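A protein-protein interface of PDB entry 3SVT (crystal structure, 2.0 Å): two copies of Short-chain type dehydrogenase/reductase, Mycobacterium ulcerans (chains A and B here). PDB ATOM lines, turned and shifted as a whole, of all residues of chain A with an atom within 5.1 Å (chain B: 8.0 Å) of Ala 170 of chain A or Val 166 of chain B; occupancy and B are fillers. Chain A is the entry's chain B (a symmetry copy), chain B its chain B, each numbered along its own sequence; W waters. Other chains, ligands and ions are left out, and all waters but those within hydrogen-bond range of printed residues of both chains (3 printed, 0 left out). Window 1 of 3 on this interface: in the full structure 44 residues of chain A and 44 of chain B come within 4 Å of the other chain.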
ATOM      1  N   VAL A 124       5.222 -26.504  27.381  1.00  0.00           N
ATOM      2  CA  VAL A 124       4.043 -25.654  27.510  1.00  0.00           C
ATOM      3  C   VAL A 124       3.384 -25.789  28.891  1.00  0.00           C
ATOM      4  O   VAL A 124       3.206 -24.814  29.605  1.00  0.00           O
ATOM      5  CB  VAL A 124       3.013 -25.933  26.382  1.00  0.00           C
ATOM      6  CG1 VAL A 124       1.877 -24.917  26.440  1.00  0.00           C
ATOM      7  CG2 VAL A 124       3.696 -25.887  25.005  1.00  0.00           C
ATOM      8  N   GLY A 165      10.628 -25.474  18.440  1.00  0.00           N
ATOM      9  CA  GLY A 165      10.391 -24.046  18.210  1.00  0.00           C
ATOM     10  C   GLY A 165       8.928 -23.664  18.401  1.00  0.00           C
ATOM     11  O   GLY A 165       8.609 -22.545  18.861  1.00  0.00           O
ATOM     12  N   VAL A 166       8.043 -24.596  18.046  1.00  0.00           N
ATOM     13  CA  VAL A 166       6.609 -24.421  18.208  1.00  0.00           C
ATOM     14  C   VAL A 166       6.309 -24.167  19.689  1.00  0.00           C
ATOM     15  O   VAL A 166       5.648 -23.179  20.046  1.00  0.00           O
ATOM     16  CB  VAL A 166       5.866 -25.684  17.736  1.00  0.00           C
ATOM     17  CG1 VAL A 166       4.408 -25.648  18.130  1.00  0.00           C
ATOM     18  CG2 VAL A 166       6.054 -25.905  16.206  1.00  0.00           C
ATOM     19  N   THR A 167       6.803 -25.037  20.563  1.00  0.00           N
ATOM     20  CA  THR A 167       6.490 -24.905  21.995  1.00  0.00           C
ATOM     21  C   THR A 167       7.227 -23.751  22.611  1.00  0.00           C
ATOM     22  O   THR A 167       6.684 -23.076  23.473  1.00  0.00           O
ATOM     23  CB  THR A 167       6.801 -26.183  22.818  1.00  0.00           C
ATOM     24  OG1 THR A 167       8.172 -26.547  22.635  1.00  0.00           O
ATOM     25  CG2 THR A 167       5.868 -27.367  22.415  1.00  0.00           C
ATOM     26  N   LYS A 168       8.466 -23.514  22.199  1.00  0.00           N
ATOM     27  CA  LYS A 168       9.213 -22.384  22.755  1.00  0.00           C
ATOM     28  C   LYS A 168       8.547 -21.051  22.349  1.00  0.00           C
ATOM     29  O   LYS A 168       8.535 -20.115  23.132  1.00  0.00           O
ATOM     30  CB  LYS A 168      10.701 -22.454  22.379  1.00  0.00           C
ATOM     31  CG  LYS A 168      11.498 -23.491  23.211  1.00  0.00           C
ATOM     32  CD  LYS A 168      11.286 -23.291  24.734  1.00  0.00           C
ATOM     33  CE  LYS A 168      12.469 -23.841  25.586  1.00  0.00           C
ATOM     34  NZ  LYS A 168      12.873 -25.232  25.227  1.00  0.00           N
ATOM     35  N   SER A 169       7.970 -20.973  21.151  1.00  0.00           N
ATOM     36  CA  SER A 169       7.126 -19.810  20.779  1.00  0.00           C
ATOM     37  C   SER A 169       5.946 -19.608  21.743  1.00  0.00           C
ATOM     38  O   SER A 169       5.635 -18.467  22.112  1.00  0.00           O
ATOM     39  CB  SER A 169       6.572 -19.930  19.368  1.00  0.00           C
ATOM     40  OG  SER A 169       7.609 -19.807  18.415  1.00  0.00           O
ATOM     41  N   ALA A 170       5.311 -20.709  22.154  1.00  0.00           N
ATOM     42  CA  ALA A 170       4.216 -20.628  23.123  1.00  0.00           C
ATOM     43  C   ALA A 170       4.691 -20.052  24.425  1.00  0.00           C
ATOM     44  O   ALA A 170       3.994 -19.248  25.062  1.00  0.00           O
ATOM     45  CB  ALA A 170       3.555 -22.010  23.403  1.00  0.00           C
ATOM     46  N   VAL A 171       5.851 -20.525  24.849  1.00  0.00           N
ATOM     47  CA  VAL A 171       6.440 -20.098  26.113  1.00  0.00           C
ATOM     48  C   VAL A 171       6.791 -18.631  26.079  1.00  0.00           C
ATOM     49  O   VAL A 171       6.581 -17.925  27.063  1.00  0.00           O
ATOM     50  CB  VAL A 171       7.683 -20.925  26.435  1.00  0.00           C
ATOM     51  CG1 VAL A 171       8.519 -20.266  27.499  1.00  0.00           C
ATOM     52  CG2 VAL A 171       7.248 -22.321  26.854  1.00  0.00           C
ATOM     53  N   ASP A 172       7.299 -18.164  24.945  1.00  0.00           N
ATOM     54  CA  ASP A 172       7.586 -16.731  24.826  1.00  0.00           C
ATOM     55  C   ASP A 172       6.315 -15.915  24.948  1.00  0.00           C
ATOM     56  O   ASP A 172       6.279 -14.913  25.670  1.00  0.00           O
ATOM     57  CB  ASP A 172       8.391 -16.426  23.560  1.00  0.00           C
ATOM     58  CG  ASP A 172       9.775 -17.067  23.613  1.00  0.00           C
ATOM     59  OD1 ASP A 172      10.351 -17.105  24.700  1.00  0.00           O
ATOM     60  OD2 ASP A 172      10.256 -17.616  22.616  1.00  0.00           O
ATOM     61  N   HIS A 173       5.244 -16.381  24.306  1.00  0.00           N
ATOM     62  CA  HIS A 173       3.993 -15.677  24.430  1.00  0.00           C
ATOM     63  C   HIS A 173       3.495 -15.676  25.882  1.00  0.00           C
ATOM     64  O   HIS A 173       2.980 -14.662  26.359  1.00  0.00           O
ATOM     65  CB  HIS A 173       2.917 -16.236  23.495  1.00  0.00           C
ATOM     66  CG  HIS A 173       1.671 -15.413  23.483  1.00  0.00           C
ATOM     67  ND1 HIS A 173       1.463 -14.395  22.583  1.00  0.00           N
ATOM     68  CD2 HIS A 173       0.590 -15.424  24.295  1.00  0.00           C
ATOM     69  CE1 HIS A 173       0.307 -13.811  22.845  1.00  0.00           C
ATOM     70  NE2 HIS A 173      -0.238 -14.410  23.884  1.00  0.00           N
ATOM     71  N   LEU A 174       3.645 -16.816  26.568  1.00  0.00           N
ATOM     72  CA  LEU A 174       3.179 -16.925  27.957  1.00  0.00           C
ATOM     73  C   LEU A 174       3.925 -15.953  28.882  1.00  0.00           C
ATOM     74  O   LEU A 174       3.323 -15.378  29.789  1.00  0.00           O
ATOM     75  CB  LEU A 174       3.303 -18.370  28.463  1.00  0.00           C
ATOM     76  CG  LEU A 174       2.974 -18.653  29.932  1.00  0.00           C
ATOM     77  CD1 LEU A 174       1.570 -18.247  30.294  1.00  0.00           C
ATOM     78  CD2 LEU A 174       3.174 -20.140  30.167  1.00  0.00           C
ATOM     79  N   LEU A 177       2.291 -12.519  28.106  1.00  0.00           N
ATOM     80  CA  LEU A 177       0.977 -12.471  28.740  1.00  0.00           C
ATOM     81  C   LEU A 177       1.080 -12.231  30.252  1.00  0.00           C
ATOM     82  O   LEU A 177       0.420 -11.334  30.795  1.00  0.00           O
ATOM     83  CB  LEU A 177       0.239 -13.775  28.479  1.00  0.00           C
ATOM     84  CG  LEU A 177      -1.153 -14.020  29.069  1.00  0.00           C
ATOM     85  CD1 LEU A 177      -2.113 -12.913  28.655  1.00  0.00           C
ATOM     86  CD2 LEU A 177      -1.656 -15.419  28.633  1.00  0.00           C
ATOM     87  N   ILE B 108      -3.722 -15.947  35.260  1.00  0.00           N
ATOM     88  CA  ILE B 108      -2.793 -17.025  35.121  1.00  0.00           C
ATOM     89  C   ILE B 108      -2.512 -17.737  36.456  1.00  0.00           C
ATOM     90  O   ILE B 108      -2.357 -18.957  36.485  1.00  0.00           O
ATOM     91  CB  ILE B 108      -1.518 -16.480  34.467  1.00  0.00           C
ATOM     92  CG1 ILE B 108      -0.737 -17.622  33.854  1.00  0.00           C
ATOM     93  CG2 ILE B 108      -0.733 -15.573  35.431  1.00  0.00           C
ATOM     94  CD1 ILE B 108      -1.466 -18.189  32.613  1.00  0.00           C
ATOM     95  N   TRP B 116      -6.766 -25.637  30.658  1.00  0.00           N
ATOM     96  CA  TRP B 116      -5.530 -25.298  29.942  1.00  0.00           C
ATOM     97  C   TRP B 116      -5.016 -26.455  29.069  1.00  0.00           C
ATOM     98  O   TRP B 116      -4.801 -26.279  27.862  1.00  0.00           O
ATOM     99  CB  TRP B 116      -4.456 -24.897  30.953  1.00  0.00           C
ATOM    100  CG  TRP B 116      -3.070 -24.699  30.389  1.00  0.00           C
ATOM    101  CD1 TRP B 116      -2.148 -25.672  30.103  1.00  0.00           C
ATOM    102  CD2 TRP B 116      -2.435 -23.447  30.092  1.00  0.00           C
ATOM    103  NE1 TRP B 116      -0.983 -25.100  29.624  1.00  0.00           N
ATOM    104  CE2 TRP B 116      -1.129 -23.740  29.612  1.00  0.00           C
ATOM    105  CE3 TRP B 116      -2.833 -22.104  30.199  1.00  0.00           C
ATOM    106  CZ2 TRP B 116      -0.231 -22.740  29.221  1.00  0.00           C
ATOM    107  CZ3 TRP B 116      -1.925 -21.111  29.817  1.00  0.00           C
ATOM    108  CH2 TRP B 116      -0.649 -21.439  29.326  1.00  0.00           C
ATOM    109  N   THR B 119      -7.266 -27.118  25.983  1.00  0.00           N
ATOM    110  CA  THR B 119      -6.923 -26.096  24.974  1.00  0.00           C
ATOM    111  C   THR B 119      -5.620 -26.378  24.231  1.00  0.00           C
ATOM    112  O   THR B 119      -5.560 -26.205  23.019  1.00  0.00           O
ATOM    113  CB  THR B 119      -6.893 -24.712  25.601  1.00  0.00           C
ATOM    114  OG1 THR B 119      -8.133 -24.520  26.264  1.00  0.00           O
ATOM    115  CG2 THR B 119      -6.733 -23.614  24.535  1.00  0.00           C
ATOM    116  N   VAL B 120      -4.577 -26.807  24.946  1.00  0.00           N
ATOM    117  CA  VAL B 120      -3.317 -27.144  24.299  1.00  0.00           C
ATOM    118  C   VAL B 120      -3.478 -28.349  23.349  1.00  0.00           C
ATOM    119  O   VAL B 120      -2.949 -28.362  22.231  1.00  0.00           O
ATOM    120  CB  VAL B 120      -2.208 -27.420  25.362  1.00  0.00           C
ATOM    121  CG1 VAL B 120      -0.993 -28.028  24.712  1.00  0.00           C
ATOM    122  CG2 VAL B 120      -1.851 -26.159  26.112  1.00  0.00           C
ATOM    123  N   ASN B 123      -5.660 -27.128  20.178  1.00  0.00           N
ATOM    124  CA  ASN B 123      -5.025 -26.162  19.303  1.00  0.00           C
ATOM    125  C   ASN B 123      -3.668 -26.628  18.797  1.00  0.00           C
ATOM    126  O   ASN B 123      -3.413 -26.590  17.594  1.00  0.00           O
ATOM    127  CB  ASN B 123      -4.895 -24.810  20.012  1.00  0.00           C
ATOM    128  CG  ASN B 123      -6.237 -24.109  20.229  1.00  0.00           C
ATOM    129  OD1 ASN B 123      -7.302 -24.584  19.824  1.00  0.00           O
ATOM    130  ND2 ASN B 123      -6.185 -22.968  20.890  1.00  0.00           N
ATOM    131  N   VAL B 124      -2.804 -27.075  19.707  1.00  0.00           N
ATOM    132  CA  VAL B 124      -1.438 -27.440  19.346  1.00  0.00           C
ATOM    133  C   VAL B 124      -1.367 -28.829  18.693  1.00  0.00           C
ATOM    134  O   VAL B 124      -0.873 -28.983  17.587  1.00  0.00           O
ATOM    135  CB  VAL B 124      -0.485 -27.361  20.570  1.00  0.00           C
ATOM    136  CG1 VAL B 124       0.959 -27.578  20.130  1.00  0.00           C
ATOM    137  CG2 VAL B 124      -0.626 -26.002  21.275  1.00  0.00           C
ATOM    138  N   ALA B 153      -5.338 -12.812  19.534  1.00  0.00           N
ATOM    139  CA  ALA B 153      -4.815 -13.206  20.831  1.00  0.00           C
ATOM    140  C   ALA B 153      -3.346 -13.640  20.755  1.00  0.00           C
ATOM    141  O   ALA B 153      -2.623 -13.486  21.734  1.00  0.00           O
ATOM    142  CB  ALA B 153      -5.692 -14.292  21.474  1.00  0.00           C
ATOM    143  N   ALA B 154      -2.903 -14.136  19.593  1.00  0.00           N
ATOM    144  CA  ALA B 154      -1.493 -14.446  19.355  1.00  0.00           C
ATOM    145  C   ALA B 154      -0.629 -13.217  19.076  1.00  0.00           C
ATOM    146  O   ALA B 154       0.555 -13.240  19.377  1.00  0.00           O
ATOM    147  CB  ALA B 154      -1.328 -15.495  18.157  1.00  0.00           C
ATOM    148  N   HIS B 158      -3.818 -10.800  25.451  1.00  0.00           N
ATOM    149  CA  HIS B 158      -5.166 -10.668  25.945  1.00  0.00           C
ATOM    150  C   HIS B 158      -5.100 -11.084  27.420  1.00  0.00           C
ATOM    151  O   HIS B 158      -5.118 -12.282  27.731  1.00  0.00           O
ATOM    152  CB  HIS B 158      -6.138 -11.600  25.191  1.00  0.00           C
ATOM    153  CG  HIS B 158      -6.498 -11.142  23.809  1.00  0.00           C
ATOM    154  ND1 HIS B 158      -5.595 -10.522  22.969  1.00  0.00           N
ATOM    155  CD2 HIS B 158      -7.661 -11.234  23.115  1.00  0.00           C
ATOM    156  CE1 HIS B 158      -6.193 -10.244  21.820  1.00  0.00           C
ATOM    157  NE2 HIS B 158      -7.445 -10.666  21.881  1.00  0.00           N
ATOM    158  N   PHE B 161      -6.770 -14.456  29.195  1.00  0.00           N
ATOM    159  CA  PHE B 161      -7.216 -15.410  28.182  1.00  0.00           C
ATOM    160  C   PHE B 161      -6.414 -16.681  28.262  1.00  0.00           C
ATOM    161  O   PHE B 161      -6.680 -17.599  27.498  1.00  0.00           O
ATOM    162  CB  PHE B 161      -7.164 -14.813  26.764  1.00  0.00           C
ATOM    163  CG  PHE B 161      -8.386 -14.003  26.403  1.00  0.00           C
ATOM    164  CD1 PHE B 161      -8.785 -12.921  27.191  1.00  0.00           C
ATOM    165  CD2 PHE B 161      -9.149 -14.331  25.293  1.00  0.00           C
ATOM    166  CE1 PHE B 161      -9.914 -12.177  26.864  1.00  0.00           C
ATOM    167  CE2 PHE B 161     -10.278 -13.581  24.948  1.00  0.00           C
ATOM    168  CZ  PHE B 161     -10.654 -12.509  25.726  1.00  0.00           C
ATOM    169  N   GLY B 162      -5.428 -16.720  29.174  1.00  0.00           N
ATOM    170  CA  GLY B 162      -4.688 -17.934  29.485  1.00  0.00           C
ATOM    171  C   GLY B 162      -4.158 -18.616  28.233  1.00  0.00           C
ATOM    172  O   GLY B 162      -3.358 -18.043  27.493  1.00  0.00           O
ATOM    173  N   ALA B 163      -4.605 -19.842  27.993  1.00  0.00           N
ATOM    174  CA  ALA B 163      -4.007 -20.701  26.951  1.00  0.00           C
ATOM    175  C   ALA B 163      -4.307 -20.274  25.502  1.00  0.00           C
ATOM    176  O   ALA B 163      -3.654 -20.721  24.577  1.00  0.00           O
ATOM    177  CB  ALA B 163      -4.451 -22.155  27.169  1.00  0.00           C
ATOM    178  N   TYR B 164      -5.331 -19.458  25.290  1.00  0.00           N
ATOM    179  CA  TYR B 164      -5.743 -19.114  23.923  1.00  0.00           C
ATOM    180  C   TYR B 164      -4.607 -18.509  23.088  1.00  0.00           C
ATOM    181  O   TYR B 164      -4.204 -19.083  22.056  1.00  0.00           O
ATOM    182  CB  TYR B 164      -6.987 -18.199  23.938  1.00  0.00           C
ATOM    183  CG  TYR B 164      -7.668 -18.064  22.571  1.00  0.00           C
ATOM    184  CD1 TYR B 164      -7.978 -19.192  21.804  1.00  0.00           C
ATOM    185  CD2 TYR B 164      -7.980 -16.814  22.045  1.00  0.00           C
ATOM    186  CE1 TYR B 164      -8.589 -19.078  20.545  1.00  0.00           C
ATOM    187  CE2 TYR B 164      -8.591 -16.690  20.791  1.00  0.00           C
ATOM    188  CZ  TYR B 164      -8.893 -17.814  20.050  1.00  0.00           C
ATOM    189  OH  TYR B 164      -9.502 -17.687  18.815  1.00  0.00           O
ATOM    190  N   GLY B 165      -4.072 -17.376  23.522  1.00  0.00           N
ATOM    191  CA  GLY B 165      -3.024 -16.703  22.747  1.00  0.00           C
ATOM    192  C   GLY B 165      -1.714 -17.482  22.746  1.00  0.00           C
ATOM    193  O   GLY B 165      -0.960 -17.474  21.748  1.00  0.00           O
ATOM    194  N   VAL B 166      -1.448 -18.154  23.867  1.00  0.00           N
ATOM    195  CA  VAL B 166      -0.269 -18.990  24.022  1.00  0.00           C
ATOM    196  C   VAL B 166      -0.288 -20.071  22.936  1.00  0.00           C
ATOM    197  O   VAL B 166       0.688 -20.242  22.189  1.00  0.00           O
ATOM    198  CB  VAL B 166      -0.268 -19.650  25.413  1.00  0.00           C
ATOM    199  CG1 VAL B 166       0.790 -20.725  25.515  1.00  0.00           C
ATOM    200  CG2 VAL B 166      -0.130 -18.583  26.538  1.00  0.00           C
ATOM    201  N   THR B 167      -1.397 -20.794  22.824  1.00  0.00           N
ATOM    202  CA  THR B 167      -1.461 -21.904  21.859  1.00  0.00           C
ATOM    203  C   THR B 167      -1.557 -21.396  20.448  1.00  0.00           C
ATOM    204  O   THR B 167      -0.984 -21.993  19.549  1.00  0.00           O
ATOM    205  CB  THR B 167      -2.641 -22.878  22.111  1.00  0.00           C
ATOM    206  OG1 THR B 167      -3.870 -22.148  22.119  1.00  0.00           O
ATOM    207  CG2 THR B 167      -2.465 -23.657  23.452  1.00  0.00           C
ATOM    208  N   LYS B 168      -2.285 -20.309  20.228  1.00  0.00           N
ATOM    209  CA  LYS B 168      -2.386 -19.764  18.872  1.00  0.00           C
ATOM    210  C   LYS B 168      -1.009 -19.253  18.397  1.00  0.00           C
ATOM    211  O   LYS B 168      -0.685 -19.380  17.226  1.00  0.00           O
ATOM    212  CB  LYS B 168      -3.491 -18.702  18.774  1.00  0.00           C
ATOM    213  CG  LYS B 168      -4.919 -19.302  18.724  1.00  0.00           C
ATOM    214  CD  LYS B 168      -5.050 -20.387  17.623  1.00  0.00           C
ATOM    215  CE  LYS B 168      -6.513 -20.564  17.119  1.00  0.00           C
ATOM    216  NZ  LYS B 168      -7.513 -20.718  18.216  1.00  0.00           N
ATOM    217  N   SER B 169      -0.193 -18.710  19.298  1.00  0.00           N
ATOM    218  CA  SER B 169       1.220 -18.399  18.965  1.00  0.00           C
ATOM    219  C   SER B 169       2.001 -19.637  18.497  1.00  0.00           C
ATOM    220  O   SER B 169       2.785 -19.551  17.541  1.00  0.00           O
ATOM    221  CB  SER B 169       1.966 -17.784  20.140  1.00  0.00           C
ATOM    222  OG  SER B 169       1.476 -16.486  20.414  1.00  0.00           O
ATOM    223  N   ALA B 170       1.771 -20.776  19.156  1.00  0.00           N
ATOM    224  CA  ALA B 170       2.416 -22.026  18.745  1.00  0.00           C
ATOM    225  C   ALA B 170       2.018 -22.402  17.348  1.00  0.00           C
ATOM    226  O   ALA B 170       2.844 -22.871  16.550  1.00  0.00           O
ATOM    227  CB  ALA B 170       2.085 -23.215  19.693  1.00  0.00           C
ATOM    228  N   VAL B 171       0.731 -22.261  17.082  1.00  0.00           N
ATOM    229  CA  VAL B 171       0.170 -22.614  15.783  1.00  0.00           C
ATOM    230  C   VAL B 171       0.725 -21.730  14.694  1.00  0.00           C
ATOM    231  O   VAL B 171       1.022 -22.212  13.602  1.00  0.00           O
ATOM    232  CB  VAL B 171      -1.354 -22.516  15.809  1.00  0.00           C
ATOM    233  CG1 VAL B 171      -1.925 -22.487  14.416  1.00  0.00           C
ATOM    234  CG2 VAL B 171      -1.908 -23.682  16.614  1.00  0.00           C
ATOM    235  N   ASP B 172       0.892 -20.448  14.992  1.00  0.00           N
ATOM    236  CA  ASP B 172       1.502 -19.556  14.000  1.00  0.00           C
ATOM    237  C   ASP B 172       2.923 -19.984  13.693  1.00  0.00           C
ATOM    238  O   ASP B 172       3.319 -20.052  12.524  1.00  0.00           O
ATOM    239  CB  ASP B 172       1.381 -18.089  14.419  1.00  0.00           C
ATOM    240  CG  ASP B 172      -0.078 -17.640  14.459  1.00  0.00           C
ATOM    241  OD1 ASP B 172      -0.842 -18.089  13.604  1.00  0.00           O
ATOM    242  OD2 ASP B 172      -0.495 -16.927  15.378  1.00  0.00           O
ATOM    243  N   HIS B 173       3.673 -20.349  14.732  1.00  0.00           N
ATOM    244  CA  HIS B 173       5.015 -20.818  14.495  1.00  0.00           C
ATOM    245  C   HIS B 173       5.017 -22.104  13.657  1.00  0.00           C
ATOM    246  O   HIS B 173       5.862 -22.264  12.773  1.00  0.00           O
ATOM    247  CB  HIS B 173       5.796 -21.024  15.796  1.00  0.00           C
ATOM    248  CG  HIS B 173       7.236 -21.342  15.567  1.00  0.00           C
ATOM    249  ND1 HIS B 173       8.211 -20.373  15.517  1.00  0.00           N
ATOM    250  CD2 HIS B 173       7.860 -22.516  15.321  1.00  0.00           C
ATOM    251  CE1 HIS B 173       9.374 -20.938  15.247  1.00  0.00           C
ATOM    252  NE2 HIS B 173       9.188 -22.237  15.114  1.00  0.00           N
HETATM  253  O   HOH W   1       3.534 -13.767  21.155  1.00  0.00           O
HETATM  254  O   HOH W   2      -2.817 -13.599  24.590  1.00  0.00           O
HETATM  255  O   HOH W   3       7.322 -17.939  15.482  1.00  0.00           O
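The backbone carbonyl oxygen (O) of Ala 153 of chain B sits close to a ring nitrogen (NE2) of His 173 of chain A, at 3.3 Å. OG of Ser 169 of chain B sits at hydrogen-bond distance from ND1 of His 173 of chain A (3.0 Å). ND1 of His 173 of chain B is in hydrogen-bond range of OG of Ser 169 of chain A (3.0 Å).
The backbone carbonyl oxygen of Gly 165 of chain B lies within hydrogen-bond range of the side-chain hydroxyl of Ser 169 of chain B. O of Gly 165 of chain A is in hydrogen-bond range of OG of Ser 169 of chain A (2.9 Å).
CG1 of Val 124 of chain A touches CG2 of Val 120 of chain B, 3.9 Å away. His 173 of chain B touches Gly 165 of chain A. Val 166 of chain A touches Ala 170 of chain B (CG1 to O, 3.6 Å). Val 166 of chain A touches His 173 of chain B (N to CD2, 3.4 Å). Val 166 of chain B touches Ala 170 of chain A (CG1 to O, 3.6 Å). CD2 of His 173 of chain A touches C of Gly 165 of chain B, at 3.5 Å. His 173 of chain A touches Val 166 of chain B (CD2 to N, 3.4 Å). Val 166 of chain B touches Leu 174 of chain A. Leu 177 of chain A touches His 158 of chain B (CD1 to O, 3.2 Å). Leu 177 of chain A touches Gly 162 of chain B (CD2 to O, 3.3 Å).
Of the printed residues of chain B, Val 124 of chain A touches Val 120. Ala 170 of chain A touches one residue of chain B. Of the printed residues of chain A, His 158 of chain B touches Leu 177. Val 166 of chain B touches three residues of chain A. The nearest residue of chain A that does not touch Val 166 of chain B is Leu 177 of chain A (4.1 Å).
Of the 22 printed residues of chain B, 11 touch a printed residue of chain A. Hydrophobic or aromatic side chains of chain B within 4 Å of the printed part of chain A: Ile 108, Val 120, Val 166, Ala 170 and His 173. Along chain B the printed residues that touch a printed residue of chain A span positions 108 to 173. Of the 12 printed residues of chain A, 8 touch a printed residue of chain B. Printed residues of chain A that touch a printed residue of chain B: Val 124, Gly 165, Val 166, Ser 169, Ala 170, His 173, Leu 174 and Leu 177. Among the printed residues, 15 pairs touch across the chains.
Gly 165 of chain A touches His 173 of chain B, and with the chains exchanged His 173 of chain A touches Gly 165 of chain B. Val 166 of chain A touches Ala 170 of chain B, and with the chains exchanged Ala 170 of chain A touches Val 166 of chain B. Val 166 of chain A touches His 173 of chain B, and with the chains exchanged His 173 of chain A touches Val 166 of chain B. Ser 169 of chain A touches His 173 of chain B, and with the chains exchanged His 173 of chain A touches Ser 169 of chain B. Positions printed for both chains: 124, 165, 166, 167, 168, 169, 170, 171, 172 and 173. Of the 15 pairs that touch across the chains among the printed residues, 8 have their exchanged pair printed and touching as well.
Water W1 bridges a ring nitrogen (ND1) of His 173 of chain A (2.6 Å) and the side-chain hydroxyl (OG) of Ser 169 of chain B (3.5 Å). Water W3 lies within hydrogen-bond range of ND1 of His 173 of chain B and OG of Ser 169 of chain A. Water W2 lies within hydrogen-bond range of NE2 of His 173 of chain A, O of Ala 153 of chain B and N of His 158 of chain B.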
